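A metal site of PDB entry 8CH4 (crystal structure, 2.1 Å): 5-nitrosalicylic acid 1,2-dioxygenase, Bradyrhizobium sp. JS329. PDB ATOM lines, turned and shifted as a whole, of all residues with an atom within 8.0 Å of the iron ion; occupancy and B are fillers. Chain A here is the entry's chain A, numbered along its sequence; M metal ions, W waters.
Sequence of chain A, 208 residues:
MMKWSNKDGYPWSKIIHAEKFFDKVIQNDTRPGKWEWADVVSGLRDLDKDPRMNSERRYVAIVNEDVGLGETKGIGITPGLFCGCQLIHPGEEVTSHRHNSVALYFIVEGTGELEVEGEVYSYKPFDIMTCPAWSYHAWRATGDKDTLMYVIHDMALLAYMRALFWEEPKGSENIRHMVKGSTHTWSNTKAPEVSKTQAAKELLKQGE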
ATOM      1  N   GLN A  86      16.153  25.292  -7.729  1.00  0.00           N
ATOM      2  CA  GLN A  86      15.851  26.264  -8.750  1.00  0.00           C
ATOM      3  C   GLN A  86      16.626  27.553  -8.501  1.00  0.00           C
ATOM      4  O   GLN A  86      16.738  27.985  -7.362  1.00  0.00           O
ATOM      5  CB  GLN A  86      14.350  26.521  -8.725  1.00  0.00           C
ATOM      6  CG  GLN A  86      13.872  27.331  -9.913  1.00  0.00           C
ATOM      7  CD  GLN A  86      12.391  27.456  -9.743  1.00  0.00           C
ATOM      8  OE1 GLN A  86      11.780  28.420 -10.169  1.00  0.00           O
ATOM      9  NE2 GLN A  86      11.813  26.463  -9.086  1.00  0.00           N
ATOM     10  N   VAL A  94       8.861  34.265 -12.615  1.00  0.00           N
ATOM     11  CA  VAL A  94       8.188  33.042 -13.008  1.00  0.00           C
ATOM     12  C   VAL A  94       6.688  33.355 -12.992  1.00  0.00           C
ATOM     13  O   VAL A  94       6.125  33.591 -11.922  1.00  0.00           O
ATOM     14  CB  VAL A  94       8.521  31.851 -12.078  1.00  0.00           C
ATOM     15  CG1 VAL A  94       7.864  30.550 -12.515  1.00  0.00           C
ATOM     16  CG2 VAL A  94      10.012  31.668 -11.843  1.00  0.00           C
ATOM     17  N   THR A  95       6.071  33.398 -14.168  1.00  0.00           N
ATOM     18  CA  THR A  95       4.716  33.930 -14.292  1.00  0.00           C
ATOM     19  C   THR A  95       3.679  32.961 -13.691  1.00  0.00           C
ATOM     20  O   THR A  95       3.974  31.792 -13.477  1.00  0.00           O
ATOM     21  CB  THR A  95       4.377  34.189 -15.760  1.00  0.00           C
ATOM     22  OG1 THR A  95       4.817  33.015 -16.428  1.00  0.00           O
ATOM     23  CG2 THR A  95       5.049  35.427 -16.307  1.00  0.00           C
ATOM     24  N   SER A  96       2.455  33.454 -13.467  1.00  0.00           N
ATOM     25  CA  SER A  96       1.410  32.676 -12.848  1.00  0.00           C
ATOM     26  C   SER A  96       1.213  31.339 -13.568  1.00  0.00           C
ATOM     27  O   SER A  96       1.248  31.262 -14.787  1.00  0.00           O
ATOM     28  CB  SER A  96       0.130  33.445 -12.776  1.00  0.00           C
ATOM     29  OG  SER A  96      -0.114  33.824 -11.432  1.00  0.00           O
ATOM     30  N   HIS A  97       1.026  30.280 -12.771  1.00  0.00           N
ATOM     31  CA  HIS A  97       0.662  28.978 -13.312  1.00  0.00           C
ATOM     32  C   HIS A  97       0.017  28.155 -12.193  1.00  0.00           C
ATOM     33  O   HIS A  97       0.025  28.584 -11.046  1.00  0.00           O
ATOM     34  CB  HIS A  97       1.858  28.334 -14.018  1.00  0.00           C
ATOM     35  CG  HIS A  97       2.893  27.738 -13.136  1.00  0.00           C
ATOM     36  ND1 HIS A  97       4.113  27.305 -13.634  1.00  0.00           N
ATOM     37  CD2 HIS A  97       2.917  27.482 -11.805  1.00  0.00           C
ATOM     38  CE1 HIS A  97       4.840  26.801 -12.653  1.00  0.00           C
ATOM     39  NE2 HIS A  97       4.126  26.902 -11.517  1.00  0.00           N
ATOM     40  N   ARG A  98      -0.565  27.012 -12.552  1.00  0.00           N
ATOM     41  CA  ARG A  98      -1.027  26.078 -11.540  1.00  0.00           C
ATOM     42  C   ARG A  98      -0.856  24.638 -12.026  1.00  0.00           C
ATOM     43  O   ARG A  98      -0.678  24.398 -13.210  1.00  0.00           O
ATOM     44  CB  ARG A  98      -2.440  26.413 -11.068  1.00  0.00           C
ATOM     45  CG  ARG A  98      -3.510  26.256 -12.135  1.00  0.00           C
ATOM     46  CD  ARG A  98      -4.760  26.914 -11.607  1.00  0.00           C
ATOM     47  NE  ARG A  98      -5.762  26.886 -12.653  1.00  0.00           N
ATOM     48  CZ  ARG A  98      -7.025  27.281 -12.515  1.00  0.00           C
ATOM     49  NH1 ARG A  98      -7.472  27.721 -11.358  1.00  0.00           N
ATOM     50  NH2 ARG A  98      -7.830  27.180 -13.541  1.00  0.00           N
ATOM     51  N   HIS A  99      -0.812  23.711 -11.071  1.00  0.00           N
ATOM     52  CA  HIS A  99      -0.697  22.276 -11.285  1.00  0.00           C
ATOM     53  C   HIS A  99      -1.236  21.636 -10.026  1.00  0.00           C
ATOM     54  O   HIS A  99      -1.198  22.258  -8.981  1.00  0.00           O
ATOM     55  CB  HIS A  99       0.763  21.857 -11.514  1.00  0.00           C
ATOM     56  CG  HIS A  99       1.748  22.683 -10.759  1.00  0.00           C
ATOM     57  ND1 HIS A  99       1.851  22.655  -9.367  1.00  0.00           N
ATOM     58  CD2 HIS A  99       2.683  23.566 -11.179  1.00  0.00           C
ATOM     59  CE1 HIS A  99       2.820  23.468  -8.976  1.00  0.00           C
ATOM     60  NE2 HIS A  99       3.350  24.038 -10.071  1.00  0.00           N
ATOM     61  N   SER A 101      -0.115  19.024  -8.613  1.00  0.00           N
ATOM     62  CA  SER A 101       1.033  18.709  -7.780  1.00  0.00           C
ATOM     63  C   SER A 101       1.287  19.870  -6.828  1.00  0.00           C
ATOM     64  O   SER A 101       1.325  21.026  -7.243  1.00  0.00           O
ATOM     65  CB  SER A 101       2.243  18.440  -8.640  1.00  0.00           C
ATOM     66  OG  SER A 101       2.217  19.253  -9.813  1.00  0.00           O
ATOM     67  N   VAL A 102       1.480  19.566  -5.535  1.00  0.00           N
ATOM     68  CA  VAL A 102       1.835  20.581  -4.554  1.00  0.00           C
ATOM     69  C   VAL A 102       3.346  20.752  -4.608  1.00  0.00           C
ATOM     70  O   VAL A 102       4.026  19.860  -5.115  1.00  0.00           O
ATOM     71  CB  VAL A 102       1.361  20.219  -3.140  1.00  0.00           C
ATOM     72  CG1 VAL A 102       2.222  19.127  -2.508  1.00  0.00           C
ATOM     73  CG2 VAL A 102       1.310  21.435  -2.240  1.00  0.00           C
ATOM     74  N   ALA A 103       3.854  21.903  -4.129  1.00  0.00           N
ATOM     75  CA  ALA A 103       5.279  22.188  -4.003  1.00  0.00           C
ATOM     76  C   ALA A 103       5.592  22.800  -2.639  1.00  0.00           C
ATOM     77  O   ALA A 103       4.797  23.553  -2.077  1.00  0.00           O
ATOM     78  CB  ALA A 103       5.771  23.039  -5.160  1.00  0.00           C
ATOM     79  N   TYR A 105       8.639  24.772  -0.586  1.00  0.00           N
ATOM     80  CA  TYR A 105       9.797  25.557  -0.944  1.00  0.00           C
ATOM     81  C   TYR A 105      10.567  25.992   0.302  1.00  0.00           C
ATOM     82  O   TYR A 105       9.973  26.451   1.287  1.00  0.00           O
ATOM     83  CB  TYR A 105       9.385  26.799  -1.731  1.00  0.00           C
ATOM     84  CG  TYR A 105       8.654  26.566  -3.035  1.00  0.00           C
ATOM     85  CD1 TYR A 105       9.345  26.306  -4.211  1.00  0.00           C
ATOM     86  CD2 TYR A 105       7.268  26.691  -3.094  1.00  0.00           C
ATOM     87  CE1 TYR A 105       8.673  26.152  -5.416  1.00  0.00           C
ATOM     88  CE2 TYR A 105       6.589  26.550  -4.292  1.00  0.00           C
ATOM     89  CZ  TYR A 105       7.292  26.277  -5.459  1.00  0.00           C
ATOM     90  OH  TYR A 105       6.601  26.128  -6.628  1.00  0.00           O
ATOM     91  N   CYS A 131       2.985  26.046  -2.024  1.00  0.00           N
ATOM     92  CA  CYS A 131       2.026  26.391  -3.064  1.00  0.00           C
ATOM     93  C   CYS A 131       1.016  25.259  -3.180  1.00  0.00           C
ATOM     94  O   CYS A 131       1.281  24.287  -3.892  1.00  0.00           O
ATOM     95  CB  CYS A 131       2.734  26.585  -4.399  1.00  0.00           C
ATOM     96  SG  CYS A 131       4.103  27.782  -4.273  1.00  0.00           S
ATOM     97  N   SER A 135      -3.222  25.853  -6.839  1.00  0.00           N
ATOM     98  CA  SER A 135      -3.177  27.284  -6.518  1.00  0.00           C
ATOM     99  C   SER A 135      -2.312  28.016  -7.539  1.00  0.00           C
ATOM    100  O   SER A 135      -1.221  27.544  -7.886  1.00  0.00           O
ATOM    101  CB  SER A 135      -2.616  27.501  -5.129  1.00  0.00           C
ATOM    102  OG  SER A 135      -3.621  27.358  -4.139  1.00  0.00           O
ATOM    103  N   TYR A 136      -2.779  29.186  -8.007  1.00  0.00           N
ATOM    104  CA  TYR A 136      -1.941  30.018  -8.867  1.00  0.00           C
ATOM    105  C   TYR A 136      -0.828  30.637  -8.028  1.00  0.00           C
ATOM    106  O   TYR A 136      -1.096  31.236  -6.964  1.00  0.00           O
ATOM    107  CB  TYR A 136      -2.745  31.137  -9.542  1.00  0.00           C
ATOM    108  CG  TYR A 136      -3.521  30.758 -10.789  1.00  0.00           C
ATOM    109  CD1 TYR A 136      -2.877  30.316 -11.936  1.00  0.00           C
ATOM    110  CD2 TYR A 136      -4.908  30.890 -10.837  1.00  0.00           C
ATOM    111  CE1 TYR A 136      -3.579  29.982 -13.087  1.00  0.00           C
ATOM    112  CE2 TYR A 136      -5.622  30.554 -11.972  1.00  0.00           C
ATOM    113  CZ  TYR A 136      -4.954  30.101 -13.101  1.00  0.00           C
ATOM    114  OH  TYR A 136      -5.662  29.759 -14.232  1.00  0.00           O
ATOM    115  N   HIS A 137       0.412  30.533  -8.529  1.00  0.00           N
ATOM    116  CA  HIS A 137       1.566  31.006  -7.805  1.00  0.00           C
ATOM    117  C   HIS A 137       2.597  31.528  -8.802  1.00  0.00           C
ATOM    118  O   HIS A 137       2.763  30.961  -9.877  1.00  0.00           O
ATOM    119  CB  HIS A 137       2.096  29.877  -6.885  1.00  0.00           C
ATOM    120  CG  HIS A 137       2.470  28.646  -7.632  1.00  0.00           C
ATOM    121  ND1 HIS A 137       1.587  27.611  -7.834  1.00  0.00           N
ATOM    122  CD2 HIS A 137       3.623  28.290  -8.264  1.00  0.00           C
ATOM    123  CE1 HIS A 137       2.185  26.672  -8.544  1.00  0.00           C
ATOM    124  NE2 HIS A 137       3.420  27.061  -8.818  1.00  0.00           N
ATOM    125  N   ALA A 138       3.307  32.606  -8.402  1.00  0.00           N
ATOM    126  CA  ALA A 138       4.300  33.269  -9.230  1.00  0.00           C
ATOM    127  C   ALA A 138       5.451  33.800  -8.368  1.00  0.00           C
ATOM    128  O   ALA A 138       5.250  34.152  -7.194  1.00  0.00           O
ATOM    129  CB  ALA A 138       3.658  34.381 -10.035  1.00  0.00           C
ATOM    130  N   TRP A 139       6.648  33.861  -8.979  1.00  0.00           N
ATOM    131  CA  TRP A 139       7.845  34.337  -8.311  1.00  0.00           C
ATOM    132  C   TRP A 139       8.421  35.586  -8.979  1.00  0.00           C
ATOM    133  O   TRP A 139       8.293  35.741 -10.194  1.00  0.00           O
ATOM    134  CB  TRP A 139       8.906  33.235  -8.281  1.00  0.00           C
ATOM    135  CG  TRP A 139       8.515  31.976  -7.574  1.00  0.00           C
ATOM    136  CD1 TRP A 139       7.898  30.898  -8.130  1.00  0.00           C
ATOM    137  CD2 TRP A 139       8.707  31.645  -6.183  1.00  0.00           C
ATOM    138  NE1 TRP A 139       7.691  29.931  -7.191  1.00  0.00           N
ATOM    139  CE2 TRP A 139       8.174  30.351  -5.987  1.00  0.00           C
ATOM    140  CE3 TRP A 139       9.255  32.318  -5.089  1.00  0.00           C
ATOM    141  CZ2 TRP A 139       8.204  29.710  -4.750  1.00  0.00           C
ATOM    142  CZ3 TRP A 139       9.279  31.684  -3.857  1.00  0.00           C
ATOM    143  CH2 TRP A 139       8.757  30.398  -3.689  1.00  0.00           C
ATOM    144  N   VAL A 151      13.326  22.330  -3.208  1.00  0.00           N
ATOM    145  CA  VAL A 151      11.903  22.186  -3.450  1.00  0.00           C
ATOM    146  C   VAL A 151      11.525  20.714  -3.398  1.00  0.00           C
ATOM    147  O   VAL A 151      12.187  19.854  -3.992  1.00  0.00           O
ATOM    148  CB  VAL A 151      11.488  22.822  -4.802  1.00  0.00           C
ATOM    149  CG1 VAL A 151      10.004  22.650  -5.065  1.00  0.00           C
ATOM    150  CG2 VAL A 151      11.889  24.304  -4.898  1.00  0.00           C
ATOM    151  N   TRP A 166      -1.597  20.262 -15.334  1.00  0.00           N
ATOM    152  CA  TRP A 166      -0.726  21.429 -15.358  1.00  0.00           C
ATOM    153  C   TRP A 166      -1.369  22.511 -16.228  1.00  0.00           C
ATOM    154  O   TRP A 166      -2.045  22.217 -17.220  1.00  0.00           O
ATOM    155  CB  TRP A 166       0.633  21.023 -15.926  1.00  0.00           C
ATOM    156  CG  TRP A 166       1.809  21.849 -15.516  1.00  0.00           C
ATOM    157  CD1 TRP A 166       2.216  23.018 -16.078  1.00  0.00           C
ATOM    158  CD2 TRP A 166       2.792  21.512 -14.520  1.00  0.00           C
ATOM    159  NE1 TRP A 166       3.386  23.441 -15.497  1.00  0.00           N
ATOM    160  CE2 TRP A 166       3.763  22.547 -14.539  1.00  0.00           C
ATOM    161  CE3 TRP A 166       2.956  20.454 -13.633  1.00  0.00           C
ATOM    162  CZ2 TRP A 166       4.861  22.561 -13.674  1.00  0.00           C
ATOM    163  CZ3 TRP A 166       4.054  20.468 -12.792  1.00  0.00           C
ATOM    164  CH2 TRP A 166       4.985  21.498 -12.805  1.00  0.00           C
ATOM    165  N   GLU A 167      -1.176  23.765 -15.831  1.00  0.00           N
ATOM    166  CA  GLU A 167      -1.751  24.878 -16.572  1.00  0.00           C
ATOM    167  C   GLU A 167      -0.731  25.996 -16.538  1.00  0.00           C
ATOM    168  O   GLU A 167      -0.609  26.725 -15.549  1.00  0.00           O
ATOM    169  CB  GLU A 167      -3.140  25.252 -16.029  1.00  0.00           C
ATOM    170  CG  GLU A 167      -3.781  26.436 -16.753  1.00  0.00           C
ATOM    171  CD  GLU A 167      -4.859  27.157 -15.967  1.00  0.00           C
ATOM    172  OE1 GLU A 167      -4.823  28.412 -15.914  1.00  0.00           O
ATOM    173  OE2 GLU A 167      -5.769  26.492 -15.402  1.00  0.00           O
ATOM    174  N   GLU A 168       0.052  26.051 -17.611  1.00  0.00           N
ATOM    175  CA  GLU A 168       1.114  27.007 -17.831  1.00  0.00           C
ATOM    176  C   GLU A 168       1.100  27.333 -19.326  1.00  0.00           C
ATOM    177  O   GLU A 168       1.018  26.439 -20.157  1.00  0.00           O
ATOM    178  CB  GLU A 168       2.449  26.392 -17.389  1.00  0.00           C
ATOM    179  CG  GLU A 168       3.680  27.213 -17.753  1.00  0.00           C
ATOM    180  CD  GLU A 168       5.000  26.705 -17.177  1.00  0.00           C
ATOM    181  OE1 GLU A 168       6.065  27.088 -17.718  1.00  0.00           O
ATOM    182  OE2 GLU A 168       4.970  25.941 -16.194  1.00  0.00           O
HETATM  183 FE    FE M   1       4.721  25.805  -9.820  1.00  0.00          FE
HETATM  184  O   HOH W   1       5.721  24.636  -8.561  1.00  0.00           O
HETATM  185  O   HOH W   2       6.424  24.999 -10.993  1.00  0.00           O
HETATM  186  O   HOH W   3       6.228  27.345 -10.007  1.00  0.00           O
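A ring nitrogen (ND1) of His 99 sits at hydrogen-bond distance from the backbone carbonyl oxygen of Ser 101, at 2.7 Å. A ring nitrogen (ND1) of His 97 lies within hydrogen-bond range of the side-chain carboxylate (OE2) of Glu 168 (3.0 Å). The backbone carbonyl oxygen (O) of Ser 135 sits at hydrogen-bond distance from a ring nitrogen (ND1) of His 137.
Tyr 105 touches the iron ion (OH to FE, 3.7 Å). Within 4 Å of the iron ion: His 97, His 99, Tyr 105 and His 137. Along chain A the residues within 4 Å of the iron ion span positions 97 to 137. The nearest printed residue that does not touch the iron ion is Trp 166 (5.0 Å).
The iron ion is bound by water W1 (2.0 Å), NE2 of His 137 (2.1 Å), NE2 of His 97 (2.1 Å), water W3 (2.2 Å), water W2 (2.2 Å) and NE2 of His 99 (2.3 Å). The iron ion has six donor atoms within binding distance.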
